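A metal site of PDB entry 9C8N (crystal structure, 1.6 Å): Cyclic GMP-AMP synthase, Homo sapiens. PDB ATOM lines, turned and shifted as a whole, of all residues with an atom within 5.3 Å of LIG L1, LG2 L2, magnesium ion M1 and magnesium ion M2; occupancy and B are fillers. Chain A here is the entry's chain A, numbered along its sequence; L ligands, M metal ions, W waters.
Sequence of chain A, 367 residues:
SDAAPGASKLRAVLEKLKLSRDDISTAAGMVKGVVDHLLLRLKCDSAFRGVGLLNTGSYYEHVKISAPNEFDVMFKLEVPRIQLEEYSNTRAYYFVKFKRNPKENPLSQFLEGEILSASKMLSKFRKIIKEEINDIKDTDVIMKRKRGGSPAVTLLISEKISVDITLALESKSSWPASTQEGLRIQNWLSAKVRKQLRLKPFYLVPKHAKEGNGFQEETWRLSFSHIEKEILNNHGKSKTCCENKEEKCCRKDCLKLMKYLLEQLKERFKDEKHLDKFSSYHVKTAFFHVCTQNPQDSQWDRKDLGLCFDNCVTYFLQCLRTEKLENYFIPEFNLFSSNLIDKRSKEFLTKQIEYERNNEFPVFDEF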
ATOM      1  N   THR A  56       8.201 -28.443  -1.328  1.00  0.00           N
ATOM      2  CA  THR A  56       8.866 -27.267  -1.921  1.00  0.00           C
ATOM      3  C   THR A  56       7.826 -26.349  -2.504  1.00  0.00           C
ATOM      4  O   THR A  56       6.632 -26.674  -2.542  1.00  0.00           O
ATOM      5  CB  THR A  56       9.833 -27.688  -3.075  1.00  0.00           C
ATOM      6  OG1 THR A  56       9.070 -28.282  -4.137  1.00  0.00           O
ATOM      7  CG2 THR A  56      10.889 -28.646  -2.547  1.00  0.00           C
ATOM      8  N   GLY A  57       8.282 -25.198  -3.014  1.00  0.00           N
ATOM      9  CA  GLY A  57       7.338 -24.373  -3.762  1.00  0.00           C
ATOM     10  C   GLY A  57       6.403 -23.547  -2.881  1.00  0.00           C
ATOM     11  O   GLY A  57       6.494 -23.494  -1.650  1.00  0.00           O
ATOM     12  N   SER A  58       5.483 -22.852  -3.565  1.00  0.00           N
ATOM     13  CA  SER A  58       4.820 -21.725  -2.903  1.00  0.00           C
ATOM     14  C   SER A  58       3.910 -22.153  -1.756  1.00  0.00           C
ATOM     15  O   SER A  58       3.762 -21.376  -0.819  1.00  0.00           O
ATOM     16  CB  SER A  58       4.029 -20.910  -3.904  1.00  0.00           C
ATOM     17  OG  SER A  58       2.926 -21.645  -4.453  1.00  0.00           O
ATOM     18  N   TYR A  59       3.276 -23.347  -1.831  1.00  0.00           N
ATOM     19  CA  TYR A  59       2.409 -23.732  -0.720  1.00  0.00           C
ATOM     20  C   TYR A  59       3.230 -23.848   0.566  1.00  0.00           C
ATOM     21  O   TYR A  59       2.863 -23.284   1.602  1.00  0.00           O
ATOM     22  CB  TYR A  59       1.726 -25.084  -1.017  1.00  0.00           C
ATOM     23  CG  TYR A  59       0.787 -25.493   0.108  1.00  0.00           C
ATOM     24  CD1 TYR A  59      -0.517 -25.080   0.151  1.00  0.00           C
ATOM     25  CD2 TYR A  59       1.252 -26.329   1.111  1.00  0.00           C
ATOM     26  CE1 TYR A  59      -1.347 -25.434   1.160  1.00  0.00           C
ATOM     27  CE2 TYR A  59       0.426 -26.684   2.203  1.00  0.00           C
ATOM     28  CZ  TYR A  59      -0.880 -26.208   2.164  1.00  0.00           C
ATOM     29  OH  TYR A  59      -1.753 -26.570   3.185  1.00  0.00           O
ATOM     30  N   GLU A  61       6.053 -22.512   1.220  1.00  0.00           N
ATOM     31  CA  GLU A  61       6.628 -21.187   1.515  1.00  0.00           C
ATOM     32  C   GLU A  61       5.583 -20.189   1.954  1.00  0.00           C
ATOM     33  O   GLU A  61       5.897 -19.034   2.224  1.00  0.00           O
ATOM     34  CB  GLU A  61       7.322 -20.651   0.246  1.00  0.00           C
ATOM     35  CG  GLU A  61       8.559 -21.510  -0.166  1.00  0.00           C
ATOM     36  CD  GLU A  61       8.957 -21.281  -1.612  1.00  0.00           C
ATOM     37  OE1 GLU A  61       8.161 -20.744  -2.407  1.00  0.00           O
ATOM     38  OE2 GLU A  61      10.115 -21.644  -1.940  1.00  0.00           O
ATOM     39  N   VAL A  63       3.404 -18.700   0.265  1.00  0.00           N
ATOM     40  CA  VAL A  63       3.126 -17.626  -0.694  1.00  0.00           C
ATOM     41  C   VAL A  63       2.239 -18.106  -1.830  1.00  0.00           C
ATOM     42  O   VAL A  63       2.043 -17.384  -2.817  1.00  0.00           O
ATOM     43  CB  VAL A  63       4.420 -16.976  -1.220  1.00  0.00           C
ATOM     44  CG1 VAL A  63       5.121 -16.224  -0.048  1.00  0.00           C
ATOM     45  CG2 VAL A  63       5.365 -17.974  -1.832  1.00  0.00           C
ATOM     46  N   LYS A  64       1.596 -19.276  -1.665  1.00  0.00           N
ATOM     47  CA  LYS A  64       0.574 -19.667  -2.643  1.00  0.00           C
ATOM     48  C   LYS A  64      -0.588 -18.677  -2.545  1.00  0.00           C
ATOM     49  O   LYS A  64      -1.002 -18.346  -1.434  1.00  0.00           O
ATOM     50  CB  LYS A  64       0.106 -21.101  -2.310  1.00  0.00           C
ATOM     51  CG  LYS A  64      -0.976 -21.665  -3.288  1.00  0.00           C
ATOM     52  CD  LYS A  64      -0.365 -22.166  -4.559  1.00  0.00           C
ATOM     53  CE  LYS A  64      -1.402 -22.591  -5.597  1.00  0.00           C
ATOM     54  NZ  LYS A  64      -2.176 -21.403  -6.138  1.00  0.00           N
ATOM     55  N   ILE A  65      -1.142 -18.261  -3.710  1.00  0.00           N
ATOM     56  CA  ILE A  65      -2.248 -17.297  -3.720  1.00  0.00           C
ATOM     57  C   ILE A  65      -3.508 -17.968  -4.243  1.00  0.00           C
ATOM     58  O   ILE A  65      -3.482 -18.945  -5.000  1.00  0.00           O
ATOM     59  CB  ILE A  65      -1.887 -16.004  -4.520  1.00  0.00           C
ATOM     60  CG1 ILE A  65      -1.548 -16.357  -5.966  1.00  0.00           C
ATOM     61  CG2 ILE A  65      -0.779 -15.229  -3.757  1.00  0.00           C
ATOM     62  CD1 ILE A  65      -1.301 -15.066  -6.807  1.00  0.00           C
ATOM     63  N   GLU A  70      -2.220 -26.146  -6.083  1.00  0.00           N
ATOM     64  CA  GLU A  70      -1.001 -26.599  -6.767  1.00  0.00           C
ATOM     65  C   GLU A  70       0.112 -26.741  -5.754  1.00  0.00           C
ATOM     66  O   GLU A  70       0.500 -25.772  -5.061  1.00  0.00           O
ATOM     67  CB  GLU A  70      -0.583 -25.610  -7.868  1.00  0.00           C
ATOM     68  CG  GLU A  70       0.316 -26.248  -8.949  1.00  0.00           C
ATOM     69  CD  GLU A  70       1.808 -26.047  -8.727  1.00  0.00           C
ATOM     70  OE1 GLU A  70       2.188 -25.367  -7.757  1.00  0.00           O
ATOM     71  OE2 GLU A  70       2.616 -26.570  -9.577  1.00  0.00           O
ATOM     72  N   PHE A  71       0.632 -27.961  -5.675  1.00  0.00           N
ATOM     73  CA  PHE A  71       1.626 -28.355  -4.677  1.00  0.00           C
ATOM     74  C   PHE A  71       2.844 -28.904  -5.398  1.00  0.00           C
ATOM     75  O   PHE A  71       2.697 -29.595  -6.402  1.00  0.00           O
ATOM     76  CB  PHE A  71       1.073 -29.472  -3.745  1.00  0.00           C
ATOM     77  CG  PHE A  71      -0.020 -29.054  -2.840  1.00  0.00           C
ATOM     78  CD1 PHE A  71      -1.313 -28.783  -3.335  1.00  0.00           C
ATOM     79  CD2 PHE A  71       0.229 -29.006  -1.470  1.00  0.00           C
ATOM     80  CE1 PHE A  71      -2.335 -28.389  -2.463  1.00  0.00           C
ATOM     81  CE2 PHE A  71      -0.788 -28.593  -0.583  1.00  0.00           C
ATOM     82  CZ  PHE A  71      -2.068 -28.306  -1.104  1.00  0.00           C
ATOM     83  N   ASP A  72       4.030 -28.681  -4.834  1.00  0.00           N
ATOM     84  CA  ASP A  72       5.290 -29.132  -5.417  1.00  0.00           C
ATOM     85  C   ASP A  72       6.063 -29.959  -4.420  1.00  0.00           C
ATOM     86  O   ASP A  72       6.276 -29.514  -3.284  1.00  0.00           O
ATOM     87  CB  ASP A  72       6.108 -27.908  -5.830  1.00  0.00           C
ATOM     88  CG  ASP A  72       5.351 -27.012  -6.791  1.00  0.00           C
ATOM     89  OD1 ASP A  72       5.180 -27.414  -7.964  1.00  0.00           O
ATOM     90  OD2 ASP A  72       4.874 -25.941  -6.312  1.00  0.00           O
ATOM     91  N   SER A 150       9.759 -30.006 -18.389  1.00  0.00           N
ATOM     92  CA  SER A 150       9.612 -30.045 -16.927  1.00  0.00           C
ATOM     93  C   SER A 150      10.306 -31.279 -16.367  1.00  0.00           C
ATOM     94  O   SER A 150      10.266 -32.360 -16.979  1.00  0.00           O
ATOM     95  CB  SER A 150       8.145 -30.088 -16.540  1.00  0.00           C
ATOM     96  OG  SER A 150       8.016 -30.290 -15.125  1.00  0.00           O
ATOM     97  N   PRO A 151      10.935 -31.174 -15.189  1.00  0.00           N
ATOM     98  CA  PRO A 151      11.485 -32.386 -14.588  1.00  0.00           C
ATOM     99  C   PRO A 151      10.447 -33.178 -13.806  1.00  0.00           C
ATOM    100  O   PRO A 151      10.781 -34.221 -13.264  1.00  0.00           O
ATOM    101  CB  PRO A 151      12.566 -31.847 -13.645  1.00  0.00           C
ATOM    102  CG  PRO A 151      11.974 -30.541 -13.145  1.00  0.00           C
ATOM    103  CD  PRO A 151      11.295 -29.966 -14.406  1.00  0.00           C
ATOM    104  N   ALA A 152       9.218 -32.673 -13.682  1.00  0.00           N
ATOM    105  CA  ALA A 152       8.212 -33.278 -12.820  1.00  0.00           C
ATOM    106  C   ALA A 152       7.313 -34.303 -13.539  1.00  0.00           C
ATOM    107  O   ALA A 152       7.142 -34.288 -14.772  1.00  0.00           O
ATOM    108  CB  ALA A 152       7.356 -32.163 -12.213  1.00  0.00           C
ATOM    109  N   ASP A 164       3.038 -31.494  -8.587  1.00  0.00           N
ATOM    110  CA  ASP A 164       4.283 -31.751  -9.323  1.00  0.00           C
ATOM    111  C   ASP A 164       5.194 -32.589  -8.449  1.00  0.00           C
ATOM    112  O   ASP A 164       5.528 -32.173  -7.328  1.00  0.00           O
ATOM    113  CB  ASP A 164       5.027 -30.457  -9.665  1.00  0.00           C
ATOM    114  CG  ASP A 164       4.328 -29.678 -10.740  1.00  0.00           C
ATOM    115  OD1 ASP A 164       3.828 -30.283 -11.727  1.00  0.00           O
ATOM    116  OD2 ASP A 164       4.274 -28.442 -10.642  1.00  0.00           O
ATOM    117  N   THR A 166       8.809 -34.176  -8.415  1.00  0.00           N
ATOM    118  CA  THR A 166      10.086 -34.107  -9.109  1.00  0.00           C
ATOM    119  C   THR A 166      11.070 -35.072  -8.471  1.00  0.00           C
ATOM    120  O   THR A 166      11.453 -34.941  -7.310  1.00  0.00           O
ATOM    121  CB  THR A 166      10.626 -32.680  -9.122  1.00  0.00           C
ATOM    122  OG1 THR A 166       9.709 -31.876  -9.838  1.00  0.00           O
ATOM    123  CG2 THR A 166      11.975 -32.609  -9.813  1.00  0.00           C
ATOM    124  N   VAL A 205      17.886 -32.573 -10.761  1.00  0.00           N
ATOM    125  CA  VAL A 205      16.542 -32.975 -11.189  1.00  0.00           C
ATOM    126  C   VAL A 205      16.635 -33.257 -12.686  1.00  0.00           C
ATOM    127  O   VAL A 205      17.506 -32.702 -13.354  1.00  0.00           O
ATOM    128  CB  VAL A 205      15.476 -31.905 -10.844  1.00  0.00           C
ATOM    129  CG1 VAL A 205      15.434 -31.648  -9.332  1.00  0.00           C
ATOM    130  CG2 VAL A 205      15.701 -30.556 -11.615  1.00  0.00           C
ATOM    131  N   LYS A 207      15.809 -32.321 -15.682  1.00  0.00           N
ATOM    132  CA  LYS A 207      15.506 -31.317 -16.679  1.00  0.00           C
ATOM    133  C   LYS A 207      16.759 -31.207 -17.534  1.00  0.00           C
ATOM    134  O   LYS A 207      17.856 -30.961 -17.002  1.00  0.00           O
ATOM    135  CB  LYS A 207      15.171 -29.970 -16.054  1.00  0.00           C
ATOM    136  CG  LYS A 207      14.984 -28.927 -17.189  1.00  0.00           C
ATOM    137  CD  LYS A 207      14.551 -27.632 -16.662  1.00  0.00           C
ATOM    138  CE  LYS A 207      14.520 -26.570 -17.767  1.00  0.00           C
ATOM    139  NZ  LYS A 207      13.595 -27.025 -18.832  1.00  0.00           N
ATOM    140  N   ARG A 221      19.812 -31.102 -13.896  1.00  0.00           N
ATOM    141  CA  ARG A 221      19.799 -29.675 -13.603  1.00  0.00           C
ATOM    142  C   ARG A 221      19.908 -29.454 -12.102  1.00  0.00           C
ATOM    143  O   ARG A 221      19.260 -30.165 -11.321  1.00  0.00           O
ATOM    144  CB  ARG A 221      18.506 -29.127 -14.173  1.00  0.00           C
ATOM    145  CG  ARG A 221      18.118 -27.775 -13.700  1.00  0.00           C
ATOM    146  CD  ARG A 221      18.961 -26.751 -14.320  1.00  0.00           C
ATOM    147  NE  ARG A 221      18.663 -25.439 -13.757  1.00  0.00           N
ATOM    148  CZ  ARG A 221      17.965 -24.469 -14.334  1.00  0.00           C
ATOM    149  NH1 ARG A 221      17.419 -24.608 -15.545  1.00  0.00           N
ATOM    150  NH2 ARG A 221      17.818 -23.319 -13.701  1.00  0.00           N
ATOM    151  N   LEU A 222      20.769 -28.520 -11.705  1.00  0.00           N
ATOM    152  CA  LEU A 222      20.920 -28.177 -10.288  1.00  0.00           C
ATOM    153  C   LEU A 222      19.636 -27.549  -9.750  1.00  0.00           C
ATOM    154  O   LEU A 222      19.029 -26.685 -10.412  1.00  0.00           O
ATOM    155  CB  LEU A 222      22.017 -27.153 -10.102  1.00  0.00           C
ATOM    156  CG  LEU A 222      23.445 -27.614 -10.173  1.00  0.00           C
ATOM    157  CD1 LEU A 222      24.377 -26.395  -9.960  1.00  0.00           C
ATOM    158  CD2 LEU A 222      23.702 -28.720  -9.089  1.00  0.00           C
ATOM    159  N   SER A 223      19.249 -27.964  -8.551  1.00  0.00           N
ATOM    160  CA  SER A 223      18.084 -27.385  -7.908  1.00  0.00           C
ATOM    161  C   SER A 223      18.394 -27.065  -6.448  1.00  0.00           C
ATOM    162  O   SER A 223      18.950 -27.898  -5.706  1.00  0.00           O
ATOM    163  CB  SER A 223      16.884 -28.329  -7.985  1.00  0.00           C
ATOM    164  OG  SER A 223      15.772 -27.804  -7.260  1.00  0.00           O
ATOM    165  N   SER A 225      15.685 -25.693  -4.519  1.00  0.00           N
ATOM    166  CA  SER A 225      14.339 -25.371  -4.046  1.00  0.00           C
ATOM    167  C   SER A 225      14.248 -25.439  -2.538  1.00  0.00           C
ATOM    168  O   SER A 225      13.495 -24.679  -1.915  1.00  0.00           O
ATOM    169  CB  SER A 225      13.294 -26.337  -4.636  1.00  0.00           C
ATOM    170  OG  SER A 225      13.256 -26.235  -6.026  1.00  0.00           O
ATOM    171  N   GLU A 228      15.543 -22.160  -1.216  1.00  0.00           N
ATOM    172  CA  GLU A 228      14.518 -21.123  -1.425  1.00  0.00           C
ATOM    173  C   GLU A 228      13.471 -21.148  -0.312  1.00  0.00           C
ATOM    174  O   GLU A 228      13.027 -20.081   0.161  1.00  0.00           O
ATOM    175  CB  GLU A 228      13.844 -21.309  -2.791  1.00  0.00           C
ATOM    176  CG  GLU A 228      14.882 -21.155  -3.892  1.00  0.00           C
ATOM    177  CD  GLU A 228      14.363 -21.510  -5.261  1.00  0.00           C
ATOM    178  OE1 GLU A 228      13.148 -21.754  -5.453  1.00  0.00           O
ATOM    179  OE2 GLU A 228      15.178 -21.560  -6.190  1.00  0.00           O
ATOM    180  N   LYS A 259       3.530 -12.095  -7.976  1.00  0.00           N
ATOM    181  CA  LYS A 259       3.011 -13.349  -8.547  1.00  0.00           C
ATOM    182  C   LYS A 259       1.648 -13.119  -9.185  1.00  0.00           C
ATOM    183  O   LYS A 259       1.394 -13.583 -10.311  1.00  0.00           O
ATOM    184  CB  LYS A 259       2.903 -14.432  -7.449  1.00  0.00           C
ATOM    185  CG  LYS A 259       4.237 -14.990  -6.978  1.00  0.00           C
ATOM    186  CD  LYS A 259       4.048 -15.770  -5.665  1.00  0.00           C
ATOM    187  CE  LYS A 259       3.077 -16.932  -5.824  1.00  0.00           C
ATOM    188  NZ  LYS A 259       3.514 -17.816  -6.905  1.00  0.00           N
ATOM    189  N   SER A 279       7.327 -17.137 -16.067  1.00  0.00           N
ATOM    190  CA  SER A 279       6.745 -17.958 -15.026  1.00  0.00           C
ATOM    191  C   SER A 279       6.899 -17.265 -13.691  1.00  0.00           C
ATOM    192  O   SER A 279       7.665 -16.302 -13.510  1.00  0.00           O
ATOM    193  CB  SER A 279       7.393 -19.361 -14.957  1.00  0.00           C
ATOM    194  OG  SER A 279       8.637 -19.277 -14.284  1.00  0.00           O
ATOM    195  N   SER A 280       6.187 -17.815 -12.686  1.00  0.00           N
ATOM    196  CA  SER A 280       6.326 -17.247 -11.355  1.00  0.00           C
ATOM    197  C   SER A 280       7.744 -17.351 -10.819  1.00  0.00           C
ATOM    198  O   SER A 280       8.099 -16.545  -9.955  1.00  0.00           O
ATOM    199  CB  SER A 280       5.336 -17.896 -10.385  1.00  0.00           C
ATOM    200  OG  SER A 280       5.599 -19.251 -10.220  1.00  0.00           O
ATOM    201  N   TYR A 281       8.575 -18.263 -11.373  1.00  0.00           N
ATOM    202  CA  TYR A 281       9.969 -18.319 -10.905  1.00  0.00           C
ATOM    203  C   TYR A 281      10.745 -17.080 -11.323  1.00  0.00           C
ATOM    204  O   TYR A 281      11.716 -16.701 -10.654  1.00  0.00           O
ATOM    205  CB  TYR A 281      10.656 -19.584 -11.443  1.00  0.00           C
ATOM    206  CG  TYR A 281      11.976 -19.855 -10.717  1.00  0.00           C
ATOM    207  CD1 TYR A 281      11.979 -20.262  -9.367  1.00  0.00           C
ATOM    208  CD2 TYR A 281      13.182 -19.700 -11.367  1.00  0.00           C
ATOM    209  CE1 TYR A 281      13.128 -20.481  -8.692  1.00  0.00           C
ATOM    210  CE2 TYR A 281      14.377 -19.972 -10.631  1.00  0.00           C
ATOM    211  CZ  TYR A 281      14.313 -20.354  -9.319  1.00  0.00           C
ATOM    212  OH  TYR A 281      15.500 -20.570  -8.688  1.00  0.00           O
ATOM    213  N   LYS A 284       9.876 -14.818  -8.567  1.00  0.00           N
ATOM    214  CA  LYS A 284      10.514 -15.261  -7.340  1.00  0.00           C
ATOM    215  C   LYS A 284      11.991 -14.880  -7.315  1.00  0.00           C
ATOM    216  O   LYS A 284      12.507 -14.368  -6.300  1.00  0.00           O
ATOM    217  CB  LYS A 284      10.356 -16.777  -7.225  1.00  0.00           C
ATOM    218  CG  LYS A 284      10.674 -17.294  -5.840  1.00  0.00           C
ATOM    219  CD  LYS A 284      10.603 -18.808  -5.854  1.00  0.00           C
ATOM    220  CE  LYS A 284      10.744 -19.332  -4.398  1.00  0.00           C
ATOM    221  NZ  LYS A 284      10.779 -20.846  -4.434  1.00  0.00           N
ATOM    222  N   ASN A 327      20.074 -16.401 -12.100  1.00  0.00           N
ATOM    223  CA  ASN A 327      19.651 -17.354 -11.106  1.00  0.00           C
ATOM    224  C   ASN A 327      20.272 -16.969  -9.756  1.00  0.00           C
ATOM    225  O   ASN A 327      21.439 -16.621  -9.698  1.00  0.00           O
ATOM    226  CB  ASN A 327      20.053 -18.757 -11.565  1.00  0.00           C
ATOM    227  CG  ASN A 327      19.562 -19.827 -10.614  1.00  0.00           C
ATOM    228  OD1 ASN A 327      20.106 -19.944  -9.541  1.00  0.00           O
ATOM    229  ND2 ASN A 327      18.532 -20.585 -10.999  1.00  0.00           N
HETATM  230  C1  LIG L   1      14.247 -26.926 -11.479  1.00  0.00           C
HETATM  231  C2  LIG L   1      12.067 -27.585 -10.665  1.00  0.00           C
HETATM  232  C3  LIG L   1      10.146 -27.031 -12.332  1.00  0.00           C
HETATM  233  C4  LIG L   1       3.233 -25.200 -12.255  1.00  0.00           C
HETATM  234  C5  LIG L   1       5.375 -26.068 -12.616  1.00  0.00           C
HETATM  235  C6  LIG L   1       6.592 -26.553 -11.801  1.00  0.00           C
HETATM  236  C7  LIG L   1       7.812 -26.831 -13.916  1.00  0.00           C
HETATM  237  C8  LIG L   1       9.033 -26.063 -14.413  1.00  0.00           C
HETATM  238  C9  LIG L   1      10.207 -26.378 -13.544  1.00  0.00           C
HETATM  239  C10 LIG L   1      12.349 -26.549 -12.833  1.00  0.00           C
HETATM  240  C11 LIG L   1      13.684 -26.474 -12.619  1.00  0.00           C
HETATM  241  C12 LIG L   1      13.416 -27.501 -10.427  1.00  0.00           C
HETATM  242  C13 LIG L   1      11.481 -27.104 -11.815  1.00  0.00           C
HETATM  243  C14 LIG L   1       8.853 -27.405 -11.674  1.00  0.00           C
HETATM  244  C15 LIG L   1       8.771 -28.977 -11.443  1.00  0.00           C
HETATM  245  N1  LIG L   1       7.729 -26.876 -12.414  1.00  0.00           N
HETATM  246  N2  LIG L   1      11.553 -26.106 -13.881  1.00  0.00           N
HETATM  247  O1  LIG L   1       4.361 -25.825 -11.687  1.00  0.00           O
HETATM  248  O2  LIG L   1       6.484 -26.714 -10.570  1.00  0.00           O
HETATM  249 CL1  LIG L   1      15.951 -26.792 -11.139  1.00  0.00          CL
HETATM  250 CL2  LIG L   1      14.641 -25.755 -13.881  1.00  0.00          CL
HETATM  251  P1  LG2 L   2       3.188 -21.098  -7.875  1.00  0.00           P
HETATM  252  O1  LG2 L   2       2.469 -20.442  -6.729  1.00  0.00           O
HETATM  253  O2  LG2 L   2       3.041 -20.447  -9.227  1.00  0.00           O
HETATM  254  O3  LG2 L   2       2.975 -22.588  -7.920  1.00  0.00           O
HETATM  255  P2  LG2 L   2       5.925 -21.861  -7.094  1.00  0.00           P
HETATM  256  O4  LG2 L   2       7.249 -21.423  -6.591  1.00  0.00           O
HETATM  257  O5  LG2 L   2       5.482 -23.195  -6.584  1.00  0.00           O
HETATM  258  N1  LG2 L   2       4.808 -20.739  -7.417  1.00  0.00           N
HETATM  259  P3  LG2 L   2       6.085 -23.672  -9.511  1.00  0.00           P
HETATM  260  O6  LG2 L   2       6.169 -23.530 -10.976  1.00  0.00           O
HETATM  261  O7  LG2 L   2       5.151 -24.690  -8.957  1.00  0.00           O
HETATM  262  O8  LG2 L   2       6.385 -22.381  -8.735  1.00  0.00           O
HETATM  263  O9  LG2 L   2       7.660 -24.506  -9.201  1.00  0.00           O
HETATM  264  C1  LG2 L   2       7.843 -25.047  -7.998  1.00  0.00           C
HETATM  265  C2  LG2 L   2       9.295 -24.865  -7.560  1.00  0.00           C
HETATM  266  O10 LG2 L   2      10.127 -25.433  -8.558  1.00  0.00           O
HETATM  267  C3  LG2 L   2       9.689 -23.380  -7.495  1.00  0.00           C
HETATM  268  O11 LG2 L   2       9.423 -22.849  -6.272  1.00  0.00           O
HETATM  269  C4  LG2 L   2      11.231 -23.521  -7.676  1.00  0.00           C
HETATM  270  O12 LG2 L   2      11.746 -23.940  -6.466  1.00  0.00           O
HETATM  271  C5  LG2 L   2      11.300 -24.699  -8.677  1.00  0.00           C
HETATM  272  N2  LG2 L   2      11.366 -24.140 -10.009  1.00  0.00           N
HETATM  273  C6  LG2 L   2      10.330 -23.820 -10.904  1.00  0.00           C
HETATM  274  N3  LG2 L   2      10.817 -23.280 -12.011  1.00  0.00           N
HETATM  275  C7  LG2 L   2      12.176 -23.234 -11.850  1.00  0.00           C
HETATM  276  C8  LG2 L   2      13.209 -22.789 -12.643  1.00  0.00           C
HETATM  277  N4  LG2 L   2      12.944 -22.265 -13.884  1.00  0.00           N
HETATM  278  N5  LG2 L   2      14.484 -22.855 -12.238  1.00  0.00           N
HETATM  279  C9  LG2 L   2      14.671 -23.377 -11.021  1.00  0.00           C
HETATM  280  N6  LG2 L   2      13.800 -23.851 -10.144  1.00  0.00           N
HETATM  281  C10 LG2 L   2      12.550 -23.754 -10.590  1.00  0.00           C
HETATM  282 MG    MG M   1       4.613 -26.635  -9.716  1.00  0.00          MG
HETATM  283 MG    MG M   2       3.858 -24.348  -7.142  1.00  0.00          MG
HETATM  284  O   HOH W   1       0.738 -22.976  -9.509  1.00  0.00           O
HETATM  285  O   HOH W   2      14.980 -25.148  -7.986  1.00  0.00           O
HETATM  286  O   HOH W   3      15.123 -20.704 -16.062  1.00  0.00           O
HETATM  287  O   HOH W   4       1.312 -22.431 -12.322  1.00  0.00           O
HETATM  288  O   HOH W   5       5.680 -29.436 -13.924  1.00  0.00           O
HETATM  289  O   HOH W   6       3.825 -21.654 -11.398  1.00  0.00           O
HETATM  290  O   HOH W   7       2.838 -24.232  -5.310  1.00  0.00           O
HETATM  291  O   HOH W   8       7.468 -21.050 -11.412  1.00  0.00           O
HETATM  292  O   HOH W   9       9.968 -28.196  -6.892  1.00  0.00           O
HETATM  293  O   HOH W  10       8.348 -19.843  -8.664  1.00  0.00           O
HETATM  294  O   HOH W  11      11.825 -24.570 -16.322  1.00  0.00           O
HETATM  295  O   HOH W  12      16.533 -21.074 -13.164  1.00  0.00           O
HETATM  296  O   HOH W  13       9.080 -22.106 -13.865  1.00  0.00           O
HETATM  297  O   HOH W  14      -0.128 -19.296  -6.377  1.00  0.00           O
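O5 of LG2 L2 sits close to N of Ser 58, at 3.0 Å. The side-chain hydroxyl (OG) of Ser 58 is in hydrogen-bond range of an oxygen (O1) of LG2 L2, at 2.6 Å. O12 of LG2 L2 lies within hydrogen-bond range of OG of Ser 225, 2.8 Å away. The side-chain carboxylate of Glu 228 lies within hydrogen-bond range of an oxygen (O12) of LG2 L2. The side-chain amino group (NZ) of Lys 259 lies within salt-bridge range of an oxygen (O1) of LG2 L2 (2.8 Å). OG of Ser 280 lies within hydrogen-bond range of O2 of LG2 L2, at 3.0 Å. An oxygen (O11) of LG2 L2 lies within hydrogen-bond range of the side-chain amino group (NZ) of Lys 284 (3.0 Å).
O of Phe 71 lies within hydrogen-bond range of N of Asp 164 (2.9 Å). The backbone carbonyl oxygen (O) of Ser 58 is in hydrogen-bond range of the backbone NH (N) of Lys 64. The side-chain hydroxyl (OG) of Ser 225 lies within hydrogen-bond range of the side-chain hydroxyl (OG) of Ser 223 (3.2 Å). The side-chain carboxylate (OE1) of Glu 228 lies within salt-bridge range of the side-chain amino group (NZ) of Lys 284 (2.7 Å). The side-chain carboxylate (OE2) of Glu 228 is in hydrogen-bond range of the side-chain hydroxyl (OH) of Tyr 281. The side-chain amino group of Lys 284 lies within salt-bridge range of the side-chain carboxylate of Glu 61 (2.7 Å). OG of Ser 279 lies close to N of Tyr 281, at 3.1 Å. N of Ala 152 sits at hydrogen-bond distance from OG of Ser 150.
Merely in contact with LIG L1: Leu 222, Lys 207, Arg 221, Thr 166, Ala 152, Ser 223, Ser 150, Pro 151 and Val 205. Hydrophobic or aromatic side chains within 4 Å of LIG L1: Pro 151, Ala 152 and Val 205. 12 residues have an atom within 4 Å of LIG L1: Glu 70, Asp 72, Ser 150, Pro 151, Ala 152, Asp 164, Thr 166, Val 205, Lys 207, Arg 221, Leu 222 and Ser 223. The nearest printed residue that does not touch LIG L1 is Ser 225 (4.6 Å).
Residues that only touch LG2 L2: Gly 57, Lys 64, Arg 221 and Tyr 281. Hydrophobic or aromatic side chains that line LG2 L2: Tyr 281. Of the 29 residues printed, 12 come within 4 Å of LG2 L2.
Within 4 Å of magnesium ion M1: Glu 70, Asp 72 and Asp 164. The nearest printed residue that does not touch magnesium ion M1 is Phe 71 (4.8 Å).
Ser 58 touches magnesium ion M2. Three residues have an atom within 4 Å of magnesium ion M2: Ser 58, Glu 70 and Asp 72. Along chain A the residues within 4 Å of magnesium ion M2 span positions 58 to 72. The nearest printed residue that does not touch magnesium ion M2 is Gly 57 (4.9 Å).
Magnesium ion M1 is bound by OD1 of Asp 72 (2.0 Å), OE2 of Glu 70 (2.0 Å), OD2 of Asp 164 (2.1 Å), O2 of LIG L1 (2.1 Å), O1 of LIG L1 (2.1 Å) and O7 of LG2 L2 (2.2 Å). Magnesium ion M1 has six donor atoms within binding distance.
Magnesium ion M2 is bound by the side-chain carboxylate of Glu 70 (2.1 Å), the side-chain carboxylate of Asp 72 (2.1 Å), an oxygen (O5) of LG2 L2 (2.1 Å), water W7 (2.1 Å), an oxygen (O3) of LG2 L2 (2.1 Å) and an oxygen (O7) of LG2 L2 (2.3 Å). Magnesium ion M2 has six donor atoms within binding distance.
Water W2 lies within hydrogen-bond range of a nitrogen (N6) of LG2 L2 (2.8 Å), the side-chain hydroxyl of Ser 225 (2.8 Å) and the side-chain hydroxyl of Ser 223 (2.9 Å). Water W10 lies within hydrogen-bond range of O4 of LG2 L2 (2.8 Å), N of Tyr 281 (3.1 Å) and OG of Ser 280 (3.2 Å). Water W8 lies within hydrogen-bond range of an oxygen (O6) of LG2 L2 (2.8 Å), the side-chain hydroxyl (OG) of Ser 280 (2.9 Å) and the backbone NH (N) of Tyr 281 (3.0 Å). Water W14 lies within hydrogen-bond range of an oxygen (O1) of LG2 L2, the side-chain amino group (NZ) of Lys 64 and the backbone NH (N) of Ile 65. Water W9 bridges OG1 of Thr 56 (2.9 Å) and O10 of LG2 L2 (3.2 Å). Water W5 bridges the side-chain hydroxyl (OG) of Ser 150 (2.8 Å) and the side-chain carboxylate (OD1) of Asp 164 (3.0 Å).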
